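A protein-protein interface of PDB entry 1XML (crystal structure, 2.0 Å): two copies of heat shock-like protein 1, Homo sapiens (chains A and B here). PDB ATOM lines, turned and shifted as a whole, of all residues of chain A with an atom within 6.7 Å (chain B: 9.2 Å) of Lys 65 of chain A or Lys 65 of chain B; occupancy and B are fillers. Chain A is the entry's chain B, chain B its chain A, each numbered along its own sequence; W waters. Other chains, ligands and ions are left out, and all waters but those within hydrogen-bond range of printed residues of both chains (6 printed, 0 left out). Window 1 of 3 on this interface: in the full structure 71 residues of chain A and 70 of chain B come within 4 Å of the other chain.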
ATOM      1  N   SER A  61      16.444  -2.526 -13.147  1.00  0.00           N
ATOM      2  CA  SER A  61      17.599  -2.706 -14.020  1.00  0.00           C
ATOM      3  C   SER A  61      18.731  -3.383 -13.248  1.00  0.00           C
ATOM      4  O   SER A  61      19.294  -2.800 -12.320  1.00  0.00           O
ATOM      5  CB  SER A  61      18.072  -1.364 -14.579  1.00  0.00           C
ATOM      6  OG  SER A  61      19.203  -1.531 -15.419  1.00  0.00           O
ATOM      7  N   ALA A  62      19.060  -4.615 -13.636  1.00  0.00           N
ATOM      8  CA  ALA A  62      20.155  -5.353 -13.011  1.00  0.00           C
ATOM      9  C   ALA A  62      21.517  -4.744 -13.352  1.00  0.00           C
ATOM     10  O   ALA A  62      22.411  -4.703 -12.501  1.00  0.00           O
ATOM     11  CB  ALA A  62      20.113  -6.823 -13.422  1.00  0.00           C
ATOM     12  N   ARG A  63      21.674  -4.278 -14.590  1.00  0.00           N
ATOM     13  CA  ARG A  63      22.939  -3.686 -15.040  1.00  0.00           C
ATOM     14  C   ARG A  63      23.240  -2.349 -14.363  1.00  0.00           C
ATOM     15  O   ARG A  63      24.385  -2.082 -13.995  1.00  0.00           O
ATOM     16  CB  ARG A  63      22.934  -3.491 -16.558  1.00  0.00           C
ATOM     17  CG  ARG A  63      22.973  -4.788 -17.354  1.00  0.00           C
ATOM     18  CD  ARG A  63      21.958  -4.846 -18.492  1.00  0.00           C
ATOM     19  NE  ARG A  63      22.403  -5.687 -19.606  1.00  0.00           N
ATOM     20  CZ  ARG A  63      23.353  -5.355 -20.484  1.00  0.00           C
ATOM     21  NH1 ARG A  63      23.992  -4.188 -20.393  1.00  0.00           N
ATOM     22  NH2 ARG A  63      23.673  -6.200 -21.462  1.00  0.00           N
ATOM     23  N   ASP A  64      22.215  -1.520 -14.202  1.00  0.00           N
ATOM     24  CA  ASP A  64      22.367  -0.191 -13.617  1.00  0.00           C
ATOM     25  C   ASP A  64      22.231  -0.198 -12.088  1.00  0.00           C
ATOM     26  O   ASP A  64      22.453   0.826 -11.446  1.00  0.00           O
ATOM     27  CB  ASP A  64      21.348   0.781 -14.229  1.00  0.00           C
ATOM     28  CG  ASP A  64      21.510   0.938 -15.739  1.00  0.00           C
ATOM     29  OD1 ASP A  64      22.436   0.327 -16.318  1.00  0.00           O
ATOM     30  OD2 ASP A  64      20.752   1.656 -16.428  1.00  0.00           O
ATOM     31  N   LYS A  65      21.884  -1.348 -11.510  1.00  0.00           N
ATOM     32  CA  LYS A  65      21.718  -1.486 -10.063  1.00  0.00           C
ATOM     33  C   LYS A  65      20.708  -0.462  -9.506  1.00  0.00           C
ATOM     34  O   LYS A  65      20.981   0.229  -8.526  1.00  0.00           O
ATOM     35  CB  LYS A  65      23.074  -1.361  -9.346  1.00  0.00           C
ATOM     36  CG  LYS A  65      24.273  -1.973 -10.080  1.00  0.00           C
ATOM     37  CD  LYS A  65      24.147  -3.474 -10.250  1.00  0.00           C
ATOM     38  CE  LYS A  65      25.364  -4.058 -10.975  1.00  0.00           C
ATOM     39  NZ  LYS A  65      25.294  -3.936 -12.447  1.00  0.00           N
ATOM     40  N   ILE A  66      19.552  -0.362 -10.163  1.00  0.00           N
ATOM     41  CA  ILE A  66      18.485   0.551  -9.745  1.00  0.00           C
ATOM     42  C   ILE A  66      17.164  -0.200  -9.658  1.00  0.00           C
ATOM     43  O   ILE A  66      16.948  -1.178 -10.376  1.00  0.00           O
ATOM     44  CB  ILE A  66      18.337   1.730 -10.746  1.00  0.00           C
ATOM     45  CG1 ILE A  66      19.662   2.474 -10.922  1.00  0.00           C
ATOM     46  CG2 ILE A  66      17.264   2.738 -10.273  1.00  0.00           C
ATOM     47  CD1 ILE A  66      19.751   3.276 -12.230  1.00  0.00           C
ATOM     48  N   ILE A  67      16.283   0.277  -8.783  1.00  0.00           N
ATOM     49  CA  ILE A  67      14.925  -0.240  -8.676  1.00  0.00           C
ATOM     50  C   ILE A  67      13.942   0.889  -8.320  1.00  0.00           C
ATOM     51  O   ILE A  67      14.249   1.761  -7.507  1.00  0.00           O
ATOM     52  CB  ILE A  67      14.882  -1.390  -7.634  1.00  0.00           C
ATOM     53  CG1 ILE A  67      15.390  -2.692  -8.276  1.00  0.00           C
ATOM     54  CG2 ILE A  67      13.483  -1.589  -7.078  1.00  0.00           C
ATOM     55  CD1 ILE A  67      15.013  -3.969  -7.542  1.00  0.00           C
ATOM     56  N   LEU A  89      15.623   3.353  -5.280  1.00  0.00           N
ATOM     57  CA  LEU A  89      16.930   3.027  -4.705  1.00  0.00           C
ATOM     58  C   LEU A  89      17.924   2.798  -5.844  1.00  0.00           C
ATOM     59  O   LEU A  89      17.619   2.090  -6.804  1.00  0.00           O
ATOM     60  CB  LEU A  89      16.849   1.762  -3.847  1.00  0.00           C
ATOM     61  CG  LEU A  89      15.938   1.673  -2.609  1.00  0.00           C
ATOM     62  CD1 LEU A  89      16.129   2.857  -1.675  1.00  0.00           C
ATOM     63  CD2 LEU A  89      14.463   1.516  -2.998  1.00  0.00           C
ATOM     64  N   GLU A  90      19.110   3.387  -5.729  1.00  0.00           N
ATOM     65  CA  GLU A  90      20.164   3.224  -6.729  1.00  0.00           C
ATOM     66  C   GLU A  90      21.524   3.083  -6.058  1.00  0.00           C
ATOM     67  O   GLU A  90      21.976   4.004  -5.390  1.00  0.00           O
ATOM     68  CB  GLU A  90      20.175   4.429  -7.665  1.00  0.00           C
ATOM     69  CG  GLU A  90      21.355   4.489  -8.624  1.00  0.00           C
ATOM     70  CD  GLU A  90      21.135   5.496  -9.741  1.00  0.00           C
ATOM     71  OE1 GLU A  90      21.702   5.312 -10.842  1.00  0.00           O
ATOM     72  OE2 GLU A  90      20.389   6.474  -9.514  1.00  0.00           O
ATOM     73  N   LYS A  91      22.177   1.939  -6.252  1.00  0.00           N
ATOM     74  CA  LYS A  91      23.529   1.718  -5.746  1.00  0.00           C
ATOM     75  C   LYS A  91      24.475   2.722  -6.387  1.00  0.00           C
ATOM     76  O   LYS A  91      24.291   3.105  -7.540  1.00  0.00           O
ATOM     77  CB  LYS A  91      24.012   0.299  -6.057  1.00  0.00           C
ATOM     78  CG  LYS A  91      23.187  -0.817  -5.407  1.00  0.00           C
ATOM     79  CD  LYS A  91      23.681  -1.161  -4.019  1.00  0.00           C
ATOM     80  CE  LYS A  91      22.778  -2.196  -3.336  1.00  0.00           C
ATOM     81  NZ  LYS A  91      23.139  -3.603  -3.699  1.00  0.00           N
ATOM     82  N   THR A  92      25.485   3.141  -5.638  1.00  0.00           N
ATOM     83  CA  THR A  92      26.372   4.206  -6.090  1.00  0.00           C
ATOM     84  C   THR A  92      27.624   3.672  -6.771  1.00  0.00           C
ATOM     85  O   THR A  92      28.037   2.533  -6.520  1.00  0.00           O
ATOM     86  CB  THR A  92      26.771   5.113  -4.915  1.00  0.00           C
ATOM     87  OG1 THR A  92      27.214   4.321  -3.800  1.00  0.00           O
ATOM     88  CG2 THR A  92      25.549   5.887  -4.407  1.00  0.00           C
ATOM     89  N   PRO A  93      28.224   4.493  -7.633  1.00  0.00           N
ATOM     90  CA  PRO A  93      29.479   4.126  -8.301  1.00  0.00           C
ATOM     91  C   PRO A  93      30.641   4.004  -7.317  1.00  0.00           C
ATOM     92  O   PRO A  93      30.644   4.671  -6.288  1.00  0.00           O
ATOM     93  CB  PRO A  93      29.729   5.296  -9.261  1.00  0.00           C
ATOM     94  CG  PRO A  93      28.433   6.009  -9.363  1.00  0.00           C
ATOM     95  CD  PRO A  93      27.753   5.826  -8.047  1.00  0.00           C
ATOM     96  N   PHE A  94      31.609   3.154  -7.637  1.00  0.00           N
ATOM     97  CA  PHE A  94      32.797   3.003  -6.803  1.00  0.00           C
ATOM     98  C   PHE A  94      33.689   4.238  -6.899  1.00  0.00           C
ATOM     99  O   PHE A  94      33.761   4.895  -7.946  1.00  0.00           O
ATOM    100  CB  PHE A  94      33.596   1.760  -7.208  1.00  0.00           C
ATOM    101  CG  PHE A  94      32.945   0.467  -6.808  1.00  0.00           C
ATOM    102  CD1 PHE A  94      32.279  -0.312  -7.747  1.00  0.00           C
ATOM    103  CD2 PHE A  94      32.999   0.032  -5.489  1.00  0.00           C
ATOM    104  CE1 PHE A  94      31.674  -1.505  -7.382  1.00  0.00           C
ATOM    105  CE2 PHE A  94      32.396  -1.163  -5.113  1.00  0.00           C
ATOM    106  CZ  PHE A  94      31.729  -1.931  -6.065  1.00  0.00           C
ATOM    107  N   ARG B  59      39.467  -0.551 -16.101  1.00  0.00           N
ATOM    108  CA  ARG B  59      38.163  -0.197 -16.675  1.00  0.00           C
ATOM    109  C   ARG B  59      37.217   0.278 -15.571  1.00  0.00           C
ATOM    110  O   ARG B  59      37.245  -0.246 -14.457  1.00  0.00           O
ATOM    111  CB  ARG B  59      37.574  -1.412 -17.406  1.00  0.00           C
ATOM    112  CG  ARG B  59      36.162  -1.243 -17.971  1.00  0.00           C
ATOM    113  CD  ARG B  59      35.571  -2.539 -18.522  1.00  0.00           C
ATOM    114  NE  ARG B  59      36.360  -3.076 -19.633  1.00  0.00           N
ATOM    115  CZ  ARG B  59      36.367  -4.352 -20.033  1.00  0.00           C
ATOM    116  NH1 ARG B  59      35.623  -5.273 -19.422  1.00  0.00           N
ATOM    117  NH2 ARG B  59      37.131  -4.712 -21.060  1.00  0.00           N
ATOM    118  N   GLU B  60      36.382   1.266 -15.882  1.00  0.00           N
ATOM    119  CA  GLU B  60      35.420   1.794 -14.913  1.00  0.00           C
ATOM    120  C   GLU B  60      34.125   2.270 -15.578  1.00  0.00           C
ATOM    121  O   GLU B  60      34.137   2.829 -16.675  1.00  0.00           O
ATOM    122  CB  GLU B  60      36.052   2.933 -14.106  1.00  0.00           C
ATOM    123  CG  GLU B  60      35.425   3.154 -12.735  1.00  0.00           C
ATOM    124  CD  GLU B  60      36.087   4.281 -11.956  1.00  0.00           C
ATOM    125  OE1 GLU B  60      37.321   4.455 -12.070  1.00  0.00           O
ATOM    126  OE2 GLU B  60      35.366   4.997 -11.223  1.00  0.00           O
ATOM    127  N   SER B  61      33.008   2.045 -14.892  1.00  0.00           N
ATOM    128  CA  SER B  61      31.694   2.428 -15.390  1.00  0.00           C
ATOM    129  C   SER B  61      30.836   2.911 -14.229  1.00  0.00           C
ATOM    130  O   SER B  61      30.550   2.150 -13.296  1.00  0.00           O
ATOM    131  CB  SER B  61      31.023   1.243 -16.086  1.00  0.00           C
ATOM    132  OG  SER B  61      29.769   1.619 -16.623  1.00  0.00           O
ATOM    133  N   ALA B  62      30.453   4.183 -14.275  1.00  0.00           N
ATOM    134  CA  ALA B  62      29.583   4.759 -13.260  1.00  0.00           C
ATOM    135  C   ALA B  62      28.160   4.256 -13.466  1.00  0.00           C
ATOM    136  O   ALA B  62      27.414   4.064 -12.500  1.00  0.00           O
ATOM    137  CB  ALA B  62      29.628   6.275 -13.324  1.00  0.00           C
ATOM    138  N   ARG B  63      27.806   4.051 -14.737  1.00  0.00           N
ATOM    139  CA  ARG B  63      26.494   3.541 -15.146  1.00  0.00           C
ATOM    140  C   ARG B  63      26.227   2.128 -14.616  1.00  0.00           C
ATOM    141  O   ARG B  63      25.140   1.848 -14.108  1.00  0.00           O
ATOM    142  CB  ARG B  63      26.402   3.538 -16.681  1.00  0.00           C
ATOM    143  CG  ARG B  63      24.996   3.370 -17.246  1.00  0.00           C
ATOM    144  CD  ARG B  63      24.978   2.964 -18.719  1.00  0.00           C
ATOM    145  NE  ARG B  63      25.304   1.548 -18.908  1.00  0.00           N
ATOM    146  CZ  ARG B  63      25.564   0.980 -20.088  1.00  0.00           C
ATOM    147  NH1 ARG B  63      25.521   1.687 -21.215  1.00  0.00           N
ATOM    148  NH2 ARG B  63      25.853  -0.314 -20.146  1.00  0.00           N
ATOM    149  N   ASP B  64      27.230   1.258 -14.739  1.00  0.00           N
ATOM    150  CA  ASP B  64      27.113  -0.156 -14.369  1.00  0.00           C
ATOM    151  C   ASP B  64      27.563  -0.452 -12.934  1.00  0.00           C
ATOM    152  O   ASP B  64      27.336  -1.550 -12.435  1.00  0.00           O
ATOM    153  CB  ASP B  64      27.921  -1.028 -15.339  1.00  0.00           C
ATOM    154  CG  ASP B  64      27.196  -1.267 -16.645  1.00  0.00           C
ATOM    155  OD1 ASP B  64      26.666  -0.295 -17.211  1.00  0.00           O
ATOM    156  OD2 ASP B  64      27.105  -2.394 -17.175  1.00  0.00           O
ATOM    157  N   LYS B  65      28.181   0.536 -12.285  1.00  0.00           N
ATOM    158  CA  LYS B  65      28.698   0.414 -10.925  1.00  0.00           C
ATOM    159  C   LYS B  65      29.661  -0.768 -10.809  1.00  0.00           C
ATOM    160  O   LYS B  65      29.477  -1.669  -9.995  1.00  0.00           O
ATOM    161  CB  LYS B  65      27.552   0.318  -9.915  1.00  0.00           C
ATOM    162  CG  LYS B  65      26.685   1.581  -9.866  1.00  0.00           C
ATOM    163  CD  LYS B  65      25.463   1.475 -10.761  1.00  0.00           C
ATOM    164  CE  LYS B  65      24.584   2.723 -10.662  1.00  0.00           C
ATOM    165  NZ  LYS B  65      23.912   3.038 -11.951  1.00  0.00           N
ATOM    166  N   ILE B  66      30.664  -0.759 -11.679  1.00  0.00           N
ATOM    167  CA  ILE B  66      31.738  -1.745 -11.666  1.00  0.00           C
ATOM    168  C   ILE B  66      33.061  -1.019 -11.852  1.00  0.00           C
ATOM    169  O   ILE B  66      33.116   0.066 -12.446  1.00  0.00           O
ATOM    170  CB  ILE B  66      31.570  -2.809 -12.796  1.00  0.00           C
ATOM    171  CG1 ILE B  66      30.141  -3.355 -12.844  1.00  0.00           C
ATOM    172  CG2 ILE B  66      32.549  -3.976 -12.596  1.00  0.00           C
ATOM    173  CD1 ILE B  66      29.812  -4.127 -14.113  1.00  0.00           C
ATOM    174  N   ILE B  67      34.120  -1.616 -11.319  1.00  0.00           N
ATOM    175  CA  ILE B  67      35.477  -1.143 -11.541  1.00  0.00           C
ATOM    176  C   ILE B  67      36.418  -2.335 -11.637  1.00  0.00           C
ATOM    177  O   ILE B  67      36.236  -3.347 -10.949  1.00  0.00           O
ATOM    178  CB  ILE B  67      35.918  -0.172 -10.421  1.00  0.00           C
ATOM    179  CG1 ILE B  67      37.197   0.561 -10.832  1.00  0.00           C
ATOM    180  CG2 ILE B  67      36.118  -0.905  -9.086  1.00  0.00           C
ATOM    181  CD1 ILE B  67      37.532   1.742  -9.943  1.00  0.00           C
ATOM    182  N   PHE B  68      37.419  -2.206 -12.501  1.00  0.00           N
ATOM    183  CA  PHE B  68      38.395  -3.256 -12.748  1.00  0.00           C
ATOM    184  C   PHE B  68      39.761  -2.698 -12.362  1.00  0.00           C
ATOM    185  O   PHE B  68      40.215  -1.702 -12.927  1.00  0.00           O
ATOM    186  CB  PHE B  68      38.387  -3.674 -14.224  1.00  0.00           C
ATOM    187  CG  PHE B  68      37.074  -4.261 -14.696  1.00  0.00           C
ATOM    188  CD1 PHE B  68      35.941  -3.463 -14.829  1.00  0.00           C
ATOM    189  CD2 PHE B  68      36.981  -5.609 -15.031  1.00  0.00           C
ATOM    190  CE1 PHE B  68      34.734  -4.003 -15.277  1.00  0.00           C
ATOM    191  CE2 PHE B  68      35.774  -6.155 -15.479  1.00  0.00           C
ATOM    192  CZ  PHE B  68      34.652  -5.349 -15.600  1.00  0.00           C
ATOM    193  N   ILE B  88      38.077  -7.198  -9.341  1.00  0.00           N
ATOM    194  CA  ILE B  88      36.891  -6.652  -9.989  1.00  0.00           C
ATOM    195  C   ILE B  88      35.763  -6.584  -8.963  1.00  0.00           C
ATOM    196  O   ILE B  88      35.332  -7.610  -8.449  1.00  0.00           O
ATOM    197  CB  ILE B  88      36.463  -7.546 -11.180  1.00  0.00           C
ATOM    198  CG1 ILE B  88      37.610  -7.700 -12.190  1.00  0.00           C
ATOM    199  CG2 ILE B  88      35.223  -6.982 -11.857  1.00  0.00           C
ATOM    200  CD1 ILE B  88      37.426  -8.851 -13.156  1.00  0.00           C
ATOM    201  N   LEU B  89      35.299  -5.377  -8.665  1.00  0.00           N
ATOM    202  CA  LEU B  89      34.194  -5.177  -7.738  1.00  0.00           C
ATOM    203  C   LEU B  89      32.979  -4.634  -8.481  1.00  0.00           C
ATOM    204  O   LEU B  89      33.086  -3.664  -9.235  1.00  0.00           O
ATOM    205  CB  LEU B  89      34.599  -4.206  -6.635  1.00  0.00           C
ATOM    206  CG  LEU B  89      35.780  -4.690  -5.785  1.00  0.00           C
ATOM    207  CD1 LEU B  89      37.095  -4.163  -6.344  1.00  0.00           C
ATOM    208  CD2 LEU B  89      35.595  -4.273  -4.334  1.00  0.00           C
ATOM    209  N   GLU B  90      31.837  -5.271  -8.257  1.00  0.00           N
ATOM    210  CA  GLU B  90      30.574  -4.881  -8.859  1.00  0.00           C
ATOM    211  C   GLU B  90      29.519  -4.811  -7.749  1.00  0.00           C
ATOM    212  O   GLU B  90      29.364  -5.759  -6.984  1.00  0.00           O
ATOM    213  CB  GLU B  90      30.173  -5.897  -9.937  1.00  0.00           C
ATOM    214  CG  GLU B  90      28.743  -5.768 -10.447  1.00  0.00           C
ATOM    215  CD  GLU B  90      28.479  -6.590 -11.699  1.00  0.00           C
ATOM    216  OE1 GLU B  90      29.001  -7.729 -11.783  1.00  0.00           O
ATOM    217  OE2 GLU B  90      27.739  -6.104 -12.591  1.00  0.00           O
ATOM    218  N   LYS B  91      28.823  -3.679  -7.652  1.00  0.00           N
ATOM    219  CA  LYS B  91      27.677  -3.555  -6.750  1.00  0.00           C
ATOM    220  C   LYS B  91      26.631  -4.544  -7.240  1.00  0.00           C
ATOM    221  O   LYS B  91      26.563  -4.830  -8.433  1.00  0.00           O
ATOM    222  CB  LYS B  91      27.098  -2.134  -6.764  1.00  0.00           C
ATOM    223  CG  LYS B  91      28.066  -1.021  -6.344  1.00  0.00           C
ATOM    224  CD  LYS B  91      28.325  -1.011  -4.841  1.00  0.00           C
ATOM    225  CE  LYS B  91      29.209   0.180  -4.425  1.00  0.00           C
ATOM    226  NZ  LYS B  91      28.433   1.434  -4.106  1.00  0.00           N
ATOM    227  N   THR B  92      25.827  -5.077  -6.336  1.00  0.00           N
ATOM    228  CA  THR B  92      24.826  -6.068  -6.723  1.00  0.00           C
ATOM    229  C   THR B  92      23.483  -5.406  -6.996  1.00  0.00           C
ATOM    230  O   THR B  92      23.182  -4.355  -6.424  1.00  0.00           O
ATOM    231  CB  THR B  92      24.646  -7.145  -5.638  1.00  0.00           C
ATOM    232  OG1 THR B  92      24.473  -6.529  -4.355  1.00  0.00           O
ATOM    233  CG2 THR B  92      25.903  -8.004  -5.499  1.00  0.00           C
ATOM    234  N   PRO B  93      22.682  -6.025  -7.862  1.00  0.00           N
ATOM    235  CA  PRO B  93      21.289  -5.609  -8.057  1.00  0.00           C
ATOM    236  C   PRO B  93      20.471  -5.769  -6.781  1.00  0.00           C
ATOM    237  O   PRO B  93      20.775  -6.633  -5.952  1.00  0.00           O
ATOM    238  CB  PRO B  93      20.762  -6.573  -9.134  1.00  0.00           C
ATOM    239  CG  PRO B  93      21.955  -7.256  -9.712  1.00  0.00           C
ATOM    240  CD  PRO B  93      23.048  -7.173  -8.714  1.00  0.00           C
ATOM    241  N   PHE B  94      19.442  -4.945  -6.629  1.00  0.00           N
ATOM    242  CA  PHE B  94      18.556  -5.033  -5.479  1.00  0.00           C
ATOM    243  C   PHE B  94      17.684  -6.278  -5.565  1.00  0.00           C
ATOM    244  O   PHE B  94      17.311  -6.712  -6.658  1.00  0.00           O
ATOM    245  CB  PHE B  94      17.655  -3.798  -5.405  1.00  0.00           C
ATOM    246  CG  PHE B  94      18.382  -2.538  -5.050  1.00  0.00           C
ATOM    247  CD1 PHE B  94      18.832  -1.678  -6.043  1.00  0.00           C
ATOM    248  CD2 PHE B  94      18.612  -2.204  -3.723  1.00  0.00           C
ATOM    249  CE1 PHE B  94      19.498  -0.509  -5.717  1.00  0.00           C
ATOM    250  CE2 PHE B  94      19.283  -1.033  -3.394  1.00  0.00           C
ATOM    251  CZ  PHE B  94      19.727  -0.189  -4.392  1.00  0.00           C
ATOM    252  N   GLN B  95      17.373  -6.849  -4.406  1.00  0.00           N
ATOM    253  CA  GLN B  95      16.361  -7.892  -4.300  1.00  0.00           C
ATOM    254  C   GLN B  95      15.117  -7.233  -3.709  1.00  0.00           C
ATOM    255  O   GLN B  95      15.216  -6.473  -2.752  1.00  0.00           O
ATOM    256  CB  GLN B  95      16.850  -9.045  -3.411  1.00  0.00           C
ATOM    257  CG  GLN B  95      18.245  -9.581  -3.764  1.00  0.00           C
ATOM    258  CD  GLN B  95      19.203  -9.591  -2.575  1.00  0.00           C
ATOM    259  OE1 GLN B  95      19.527  -8.539  -2.017  1.00  0.00           O
ATOM    260  NE2 GLN B  95      19.657 -10.778  -2.190  1.00  0.00           N
ATOM    261  N   VAL B  99      14.411  -4.941   0.141  1.00  0.00           N
ATOM    262  CA  VAL B  99      14.182  -3.501   0.052  1.00  0.00           C
ATOM    263  C   VAL B  99      12.900  -3.122   0.796  1.00  0.00           C
ATOM    264  O   VAL B  99      12.899  -2.182   1.584  1.00  0.00           O
ATOM    265  CB  VAL B  99      14.101  -3.004  -1.416  1.00  0.00           C
ATOM    266  CG1 VAL B  99      13.667  -1.542  -1.471  1.00  0.00           C
ATOM    267  CG2 VAL B  99      15.441  -3.179  -2.119  1.00  0.00           C
ATOM    268  N   LEU B 129      22.160  -5.918   2.193  1.00  0.00           N
ATOM    269  CA  LEU B 129      21.978  -5.194   0.929  1.00  0.00           C
ATOM    270  C   LEU B 129      23.290  -4.639   0.336  1.00  0.00           C
ATOM    271  O   LEU B 129      23.293  -4.085  -0.774  1.00  0.00           O
ATOM    272  CB  LEU B 129      21.004  -4.022   1.131  1.00  0.00           C
ATOM    273  CG  LEU B 129      19.574  -4.314   1.606  1.00  0.00           C
ATOM    274  CD1 LEU B 129      19.497  -4.689   3.083  1.00  0.00           C
ATOM    275  CD2 LEU B 129      18.679  -3.109   1.315  1.00  0.00           C
ATOM    276  N   ASP B 131      26.149  -6.293  -0.396  1.00  0.00           N
ATOM    277  CA  ASP B 131      27.009  -7.294  -1.027  1.00  0.00           C
ATOM    278  C   ASP B 131      27.628  -6.766  -2.331  1.00  0.00           C
ATOM    279  O   ASP B 131      26.929  -6.238  -3.189  1.00  0.00           O
ATOM    280  CB  ASP B 131      26.224  -8.592  -1.280  1.00  0.00           C
ATOM    281  CG  ASP B 131      27.088  -9.708  -1.865  1.00  0.00           C
ATOM    282  OD1 ASP B 131      28.336  -9.600  -1.846  1.00  0.00           O
ATOM    283  OD2 ASP B 131      26.596 -10.742  -2.370  1.00  0.00           O
ATOM    284  N   VAL B 132      28.946  -6.913  -2.455  1.00  0.00           N
ATOM    285  CA  VAL B 132      29.681  -6.547  -3.662  1.00  0.00           C
ATOM    286  C   VAL B 132      30.315  -7.809  -4.252  1.00  0.00           C
ATOM    287  O   VAL B 132      31.161  -8.431  -3.616  1.00  0.00           O
ATOM    288  CB  VAL B 132      30.772  -5.484  -3.351  1.00  0.00           C
ATOM    289  CG1 VAL B 132      31.758  -5.337  -4.507  1.00  0.00           C
ATOM    290  CG2 VAL B 132      30.131  -4.136  -3.031  1.00  0.00           C
ATOM    291  N   LYS B 133      29.896  -8.190  -5.456  1.00  0.00           N
ATOM    292  CA  LYS B 133      30.522  -9.307  -6.170  1.00  0.00           C
ATOM    293  C   LYS B 133      31.969  -8.950  -6.532  1.00  0.00           C
ATOM    294  O   LYS B 133      32.225  -7.936  -7.187  1.00  0.00           O
ATOM    295  CB  LYS B 133      29.736  -9.674  -7.435  1.00  0.00           C
ATOM    296  CG  LYS B 133      28.242  -9.918  -7.204  1.00  0.00           C
ATOM    297  CD  LYS B 133      27.791 -11.292  -7.701  1.00  0.00           C
ATOM    298  CE  LYS B 133      26.282 -11.475  -7.541  1.00  0.00           C
ATOM    299  NZ  LYS B 133      25.504 -10.410  -8.245  1.00  0.00           N
HETATM  300  O   HOH W   1      32.171   2.479 -10.713  1.00  0.00           O
HETATM  301  O   HOH W   2      25.974  -3.696  -3.436  1.00  0.00           O
HETATM  302  O   HOH W   3      21.492  -5.601  -3.214  1.00  0.00           O
HETATM  303  O   HOH W   4      30.595   3.207  -3.339  1.00  0.00           O
HETATM  304  O   HOH W   5      23.387  -1.196 -18.788  1.00  0.00           O
HETATM  305  O   HOH W   6      18.530  -3.747  -9.380  1.00  0.00           O
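O of Asp 64 of chain A lies within hydrogen-bond range of NZ of Lys 65 of chain B (2.7 Å). The side-chain amino group of Lys 65 of chain A sits at hydrogen-bond distance from the backbone carbonyl oxygen of Asp 64 of chain B (3.1 Å). The side-chain amino group (NZ) of Lys 65 of chain A is in salt-bridge range of the side-chain carboxylate (OE2) of Glu 90 of chain B (3.3 Å). The side-chain carboxylate of Glu 90 of chain A lies within salt-bridge range of the side-chain amino group of Lys 65 of chain B (3.4 Å). The backbone carbonyl oxygen (O) of Thr 92 of chain B is in hydrogen-bond range of the side-chain amino group (NZ) of Lys 91 of chain A (2.8 Å). The side-chain amino group (NZ) of Lys 91 of chain A is in hydrogen-bond range of the backbone carbonyl oxygen (O) of Leu 129 of chain B (3.0 Å). O of Thr 92 of chain A lies within hydrogen-bond range of NZ of Lys 91 of chain B, at 2.7 Å. O of Arg 63 of chain A lies close to O of Asp 64 of chain B (3.4 Å).
The side-chain hydroxyl (OG) of Ser 61 of chain B sits at hydrogen-bond distance from the backbone NH (N) of Asp 64 of chain B, 3.2 Å away.
Of the printed residues of chain B, Glu 90 of chain A touches Lys 65 (3.4 Å) and Phe 94 (3.9 Å). Ser 61 of chain B touches none of the printed residues of chain A. Of chain A, only Asp 64 (2.7 Å), Lys 65 (3.7 Å), Glu 90 (3.4 Å), Lys 91 (3.2 Å), Thr 92 (3.7 Å), Pro 93 (3.98 Å) and Phe 94 (3.4 Å) come within 4 Å of Lys 65 of chain B. Printed residues of chain A within 4 Å of Pro 93 of chain B: Ala 62 and Lys 65. The nearest residue of chain A that does not touch Lys 65 of chain B is Ile 66 of chain A (4.2 Å). The nearest printed residue of chain B that does not touch Ala 62 of chain A is Glu 90 of chain B (5.5 Å).
Of the 23 printed residues of chain B, 14 touch a printed residue of chain A. Hydrophobic or aromatic side chains of chain B that line the printed part of chain A: Leu 89, Pro 93, Phe 94, Val 99 and Val 132.
Lys 65 of chain B touches its own counterpart, Lys 65 of chain A. Lys 91 of chain A touches Thr 92 of chain B, and with the chains exchanged Thr 92 of chain A touches Lys 91 of chain B.
Water W2 lies within hydrogen-bond range of the backbone carbonyl oxygen of Asp 131 of chain B (2.7 Å), the side-chain amino group of Lys 91 of chain A (2.8 Å) and the backbone NH of Thr 92 of chain B (3.2 Å).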
